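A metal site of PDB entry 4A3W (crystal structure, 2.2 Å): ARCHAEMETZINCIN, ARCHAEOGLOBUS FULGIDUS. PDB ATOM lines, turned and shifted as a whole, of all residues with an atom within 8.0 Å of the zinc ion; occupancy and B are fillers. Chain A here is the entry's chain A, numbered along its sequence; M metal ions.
The backbone NH of Cys 128 sits at hydrogen-bond distance from the backbone carbonyl oxygen of Met 134 (3.2 Å).
The side-chain sulfur (SG) of Cys 132 lies close to the backbone NH (N) of Met 134, at 3.4 Å.
SG of Cys 128 lies close to N of Asn 130 (3.3 Å).
The side-chain sulfur (SG) of Cys 151 lies close to the side-chain amide nitrogen (ND2) of Asn 130, at 3.3 Å.
The side-chain sulfur of Cys 151 lies close to the backbone NH of Glu 153, 3.6 Å away.
Four residues have an atom within 4 Å of the zinc ion: Cys 128, Cys 132, Cys 151 and Cys 154.
The nearest printed residue that does not touch the zinc ion is Asn 130 (4.2 Å).
The side-chain sulfur (SG) of Cys 154 binds the zinc ion.
The zinc ion is bound by the side-chain sulfur (SG) of Cys 132, 2.3 Å away.
The zinc ion is bound by the side-chain sulfur (SG) of Cys 151 (2.4 Å).
The zinc ion is bound by SG of Cys 128 (2.4 Å).
The zinc ion has four donor atoms within binding distance.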
ATOM      1  N   LEU A 125     -18.341  23.747  30.275  1.00  0.00           N
ATOM      2  CA  LEU A 125     -16.992  23.146  30.327  1.00  0.00           C
ATOM      3  C   LEU A 125     -16.502  22.962  31.750  1.00  0.00           C
ATOM      4  O   LEU A 125     -16.597  23.873  32.596  1.00  0.00           O
ATOM      5  CB  LEU A 125     -15.978  23.984  29.542  1.00  0.00           C
ATOM      6  CG  LEU A 125     -16.193  24.157  28.034  1.00  0.00           C
ATOM      7  CD1 LEU A 125     -15.177  25.138  27.430  1.00  0.00           C
ATOM      8  CD2 LEU A 125     -16.134  22.815  27.315  1.00  0.00           C
ATOM      9  N   LYS A 126     -15.960  21.788  32.026  1.00  0.00           N
ATOM     10  CA  LYS A 126     -15.315  21.540  33.306  1.00  0.00           C
ATOM     11  C   LYS A 126     -13.823  21.863  33.191  1.00  0.00           C
ATOM     12  O   LYS A 126     -13.343  22.231  32.119  1.00  0.00           O
ATOM     13  CB  LYS A 126     -15.466  20.079  33.724  1.00  0.00           C
ATOM     14  CG  LYS A 126     -16.903  19.643  33.967  1.00  0.00           C
ATOM     15  CD  LYS A 126     -16.959  18.169  34.370  1.00  0.00           C
ATOM     16  CE  LYS A 126     -18.269  17.521  33.970  1.00  0.00           C
ATOM     17  NZ  LYS A 126     -18.110  16.047  33.739  1.00  0.00           N
ATOM     18  N   HIS A 127     -13.100  21.692  34.274  1.00  0.00           N
ATOM     19  CA  HIS A 127     -11.673  21.894  34.224  1.00  0.00           C
ATOM     20  C   HIS A 127     -10.994  20.926  33.254  1.00  0.00           C
ATOM     21  O   HIS A 127     -11.448  19.799  33.030  1.00  0.00           O
ATOM     22  CB  HIS A 127     -11.074  21.797  35.618  1.00  0.00           C
ATOM     23  CG  HIS A 127     -11.369  23.014  36.451  1.00  0.00           C
ATOM     24  ND1 HIS A 127     -11.499  22.968  37.819  1.00  0.00           N
ATOM     25  CD2 HIS A 127     -11.572  24.298  36.090  1.00  0.00           C
ATOM     26  CE1 HIS A 127     -11.788  24.162  38.267  1.00  0.00           C
ATOM     27  NE2 HIS A 127     -11.836  24.991  37.246  1.00  0.00           N
ATOM     28  N   CYS A 128      -9.911  21.417  32.662  1.00  0.00           N
ATOM     29  CA  CYS A 128      -9.215  20.722  31.592  1.00  0.00           C
ATOM     30  C   CYS A 128      -7.767  20.582  32.010  1.00  0.00           C
ATOM     31  O   CYS A 128      -7.210  21.494  32.625  1.00  0.00           O
ATOM     32  CB  CYS A 128      -9.317  21.557  30.322  1.00  0.00           C
ATOM     33  SG  CYS A 128      -8.508  20.861  28.893  1.00  0.00           S
ATOM     34  N   SER A 129      -7.124  19.467  31.690  1.00  0.00           N
ATOM     35  CA  SER A 129      -5.707  19.313  32.016  1.00  0.00           C
ATOM     36  C   SER A 129      -4.806  19.565  30.815  1.00  0.00           C
ATOM     37  O   SER A 129      -3.587  19.441  30.912  1.00  0.00           O
ATOM     38  CB  SER A 129      -5.419  17.928  32.587  1.00  0.00           C
ATOM     39  OG  SER A 129      -5.660  16.926  31.618  1.00  0.00           O
ATOM     40  N   ASN A 130      -5.398  19.936  29.683  1.00  0.00           N
ATOM     41  CA  ASN A 130      -4.590  20.298  28.525  1.00  0.00           C
ATOM     42  C   ASN A 130      -4.080  21.714  28.665  1.00  0.00           C
ATOM     43  O   ASN A 130      -4.363  22.397  29.664  1.00  0.00           O
ATOM     44  CB  ASN A 130      -5.382  20.151  27.216  1.00  0.00           C
ATOM     45  CG  ASN A 130      -6.024  18.795  27.082  1.00  0.00           C
ATOM     46  OD1 ASN A 130      -5.462  17.794  27.529  1.00  0.00           O
ATOM     47  ND2 ASN A 130      -7.204  18.746  26.474  1.00  0.00           N
ATOM     48  N   ASN A 131      -3.308  22.158  27.678  1.00  0.00           N
ATOM     49  CA  ASN A 131      -2.824  23.522  27.624  1.00  0.00           C
ATOM     50  C   ASN A 131      -3.977  24.392  27.168  1.00  0.00           C
ATOM     51  O   ASN A 131      -4.197  24.581  25.963  1.00  0.00           O
ATOM     52  CB  ASN A 131      -1.649  23.619  26.657  1.00  0.00           C
ATOM     53  CG  ASN A 131      -1.033  25.000  26.643  1.00  0.00           C
ATOM     54  OD1 ASN A 131      -0.746  25.576  27.696  1.00  0.00           O
ATOM     55  ND2 ASN A 131      -0.842  25.544  25.445  1.00  0.00           N
ATOM     56  N   CYS A 132      -4.721  24.918  28.118  1.00  0.00           N
ATOM     57  CA  CYS A 132      -6.058  25.392  27.815  1.00  0.00           C
ATOM     58  C   CYS A 132      -6.498  26.400  28.851  1.00  0.00           C
ATOM     59  O   CYS A 132      -6.163  26.265  30.028  1.00  0.00           O
ATOM     60  CB  CYS A 132      -7.010  24.179  27.812  1.00  0.00           C
ATOM     61  SG  CYS A 132      -8.778  24.526  27.524  1.00  0.00           S
ATOM     62  N   VAL A 133      -7.243  27.408  28.407  1.00  0.00           N
ATOM     63  CA  VAL A 133      -7.780  28.409  29.315  1.00  0.00           C
ATOM     64  C   VAL A 133      -8.633  27.762  30.428  1.00  0.00           C
ATOM     65  O   VAL A 133      -8.785  28.344  31.510  1.00  0.00           O
ATOM     66  CB  VAL A 133      -8.606  29.473  28.540  1.00  0.00           C
ATOM     67  CG1 VAL A 133      -9.947  28.870  28.015  1.00  0.00           C
ATOM     68  CG2 VAL A 133      -8.849  30.710  29.411  1.00  0.00           C
ATOM     69  N   MET A 134      -9.152  26.556  30.189  1.00  0.00           N
ATOM     70  CA  MET A 134     -10.017  25.896  31.189  1.00  0.00           C
ATOM     71  C   MET A 134      -9.240  25.152  32.304  1.00  0.00           C
ATOM     72  O   MET A 134      -9.832  24.550  33.215  1.00  0.00           O
ATOM     73  CB  MET A 134     -11.007  24.927  30.520  1.00  0.00           C
ATOM     74  CG  MET A 134     -12.123  25.614  29.718  1.00  0.00           C
ATOM     75  SD  MET A 134     -12.937  26.946  30.635  1.00  0.00           S
ATOM     76  CE  MET A 134     -13.420  26.119  32.154  1.00  0.00           C
ATOM     77  N   ARG A 135      -7.926  25.220  32.257  1.00  0.00           N
ATOM     78  CA  ARG A 135      -7.095  24.692  33.325  1.00  0.00           C
ATOM     79  C   ARG A 135      -7.415  25.431  34.622  1.00  0.00           C
ATOM     80  O   ARG A 135      -7.627  26.642  34.619  1.00  0.00           O
ATOM     81  CB  ARG A 135      -5.622  24.881  32.950  1.00  0.00           C
ATOM     82  CG  ARG A 135      -4.650  24.172  33.843  1.00  0.00           C
ATOM     83  CD  ARG A 135      -3.218  24.390  33.382  1.00  0.00           C
ATOM     84  NE  ARG A 135      -2.865  23.530  32.258  1.00  0.00           N
ATOM     85  CZ  ARG A 135      -1.698  23.588  31.614  1.00  0.00           C
ATOM     86  NH1 ARG A 135      -0.774  24.471  31.962  1.00  0.00           N
ATOM     87  NH2 ARG A 135      -1.465  22.754  30.606  1.00  0.00           N
ATOM     88  N   SER A 149      -6.578  30.643  25.045  1.00  0.00           N
ATOM     89  CA  SER A 149      -7.334  29.853  24.060  1.00  0.00           C
ATOM     90  C   SER A 149      -7.849  28.533  24.619  1.00  0.00           C
ATOM     91  O   SER A 149      -7.256  27.953  25.520  1.00  0.00           O
ATOM     92  CB  SER A 149      -6.441  29.575  22.841  1.00  0.00           C
ATOM     93  OG  SER A 149      -5.202  29.013  23.249  1.00  0.00           O
ATOM     94  N   PHE A 150      -8.978  28.067  24.081  1.00  0.00           N
ATOM     95  CA  PHE A 150      -9.465  26.713  24.356  1.00  0.00           C
ATOM     96  C   PHE A 150      -8.683  25.683  23.550  1.00  0.00           C
ATOM     97  O   PHE A 150      -8.395  25.908  22.386  1.00  0.00           O
ATOM     98  CB  PHE A 150     -10.946  26.588  23.960  1.00  0.00           C
ATOM     99  CG  PHE A 150     -11.858  27.467  24.755  1.00  0.00           C
ATOM    100  CD1 PHE A 150     -12.282  27.072  26.020  1.00  0.00           C
ATOM    101  CD2 PHE A 150     -12.281  28.693  24.250  1.00  0.00           C
ATOM    102  CE1 PHE A 150     -13.116  27.895  26.773  1.00  0.00           C
ATOM    103  CE2 PHE A 150     -13.115  29.513  24.993  1.00  0.00           C
ATOM    104  CZ  PHE A 150     -13.534  29.109  26.262  1.00  0.00           C
ATOM    105  N   CYS A 151      -8.340  24.563  24.163  1.00  0.00           N
ATOM    106  CA  CYS A 151      -7.719  23.464  23.411  1.00  0.00           C
ATOM    107  C   CYS A 151      -8.750  22.925  22.412  1.00  0.00           C
ATOM    108  O   CYS A 151      -9.932  23.242  22.511  1.00  0.00           O
ATOM    109  CB  CYS A 151      -7.260  22.357  24.363  1.00  0.00           C
ATOM    110  SG  CYS A 151      -8.633  21.410  25.106  1.00  0.00           S
ATOM    111  N   ARG A 152      -8.320  22.097  21.448  1.00  0.00           N
ATOM    112  CA  ARG A 152      -9.221  21.542  20.437  1.00  0.00           C
ATOM    113  C   ARG A 152     -10.395  20.779  21.020  1.00  0.00           C
ATOM    114  O   ARG A 152     -11.503  20.830  20.473  1.00  0.00           O
ATOM    115  CB  ARG A 152      -8.462  20.635  19.447  1.00  0.00           C
ATOM    116  CG  ARG A 152      -7.521  21.407  18.502  1.00  0.00           C
ATOM    117  CD  ARG A 152      -6.903  20.471  17.455  1.00  0.00           C
ATOM    118  NE  ARG A 152      -6.040  19.460  18.063  1.00  0.00           N
ATOM    119  CZ  ARG A 152      -6.282  18.157  18.047  1.00  0.00           C
ATOM    120  NH1 ARG A 152      -7.361  17.663  17.456  1.00  0.00           N
ATOM    121  NH2 ARG A 152      -5.432  17.322  18.631  1.00  0.00           N
ATOM    122  N   GLU A 153     -10.191  20.072  22.128  1.00  0.00           N
ATOM    123  CA  GLU A 153     -11.308  19.344  22.753  1.00  0.00           C
ATOM    124  C   GLU A 153     -12.349  20.297  23.325  1.00  0.00           C
ATOM    125  O   GLU A 153     -13.531  20.120  23.084  1.00  0.00           O
ATOM    126  CB  GLU A 153     -10.825  18.395  23.861  1.00  0.00           C
ATOM    127  CG  GLU A 153     -10.087  17.179  23.325  1.00  0.00           C
ATOM    128  CD  GLU A 153      -9.661  16.204  24.420  1.00  0.00           C
ATOM    129  OE1 GLU A 153      -9.237  16.655  25.512  1.00  0.00           O
ATOM    130  OE2 GLU A 153      -9.723  14.983  24.165  1.00  0.00           O
ATOM    131  N   CYS A 154     -11.921  21.292  24.098  1.00  0.00           N
ATOM    132  CA  CYS A 154     -12.885  22.191  24.703  1.00  0.00           C
ATOM    133  C   CYS A 154     -13.589  23.029  23.630  1.00  0.00           C
ATOM    134  O   CYS A 154     -14.791  23.269  23.715  1.00  0.00           O
ATOM    135  CB  CYS A 154     -12.221  23.080  25.767  1.00  0.00           C
ATOM    136  SG  CYS A 154     -11.700  22.183  27.272  1.00  0.00           S
ATOM    137  N   ALA A 155     -12.861  23.461  22.615  1.00  0.00           N
ATOM    138  CA  ALA A 155     -13.453  24.254  21.540  1.00  0.00           C
ATOM    139  C   ALA A 155     -14.544  23.449  20.819  1.00  0.00           C
ATOM    140  O   ALA A 155     -15.564  24.008  20.428  1.00  0.00           O
ATOM    141  CB  ALA A 155     -12.394  24.710  20.545  1.00  0.00           C
ATOM    142  N   LYS A 157     -16.550  21.333  22.062  1.00  0.00           N
ATOM    143  CA  LYS A 157     -17.712  21.129  22.919  1.00  0.00           C
ATOM    144  C   LYS A 157     -18.606  22.369  23.048  1.00  0.00           C
ATOM    145  O   LYS A 157     -19.698  22.266  23.592  1.00  0.00           O
ATOM    146  CB  LYS A 157     -17.282  20.696  24.315  1.00  0.00           C
ATOM    147  CG  LYS A 157     -16.635  19.344  24.414  1.00  0.00           C
ATOM    148  CD  LYS A 157     -16.078  19.172  25.802  1.00  0.00           C
ATOM    149  CE  LYS A 157     -15.704  17.737  26.117  1.00  0.00           C
ATOM    150  NZ  LYS A 157     -14.461  17.318  25.438  1.00  0.00           N
HETATM  151 ZN    ZN M   1      -9.393  22.289  27.194  1.00  0.00          ZN
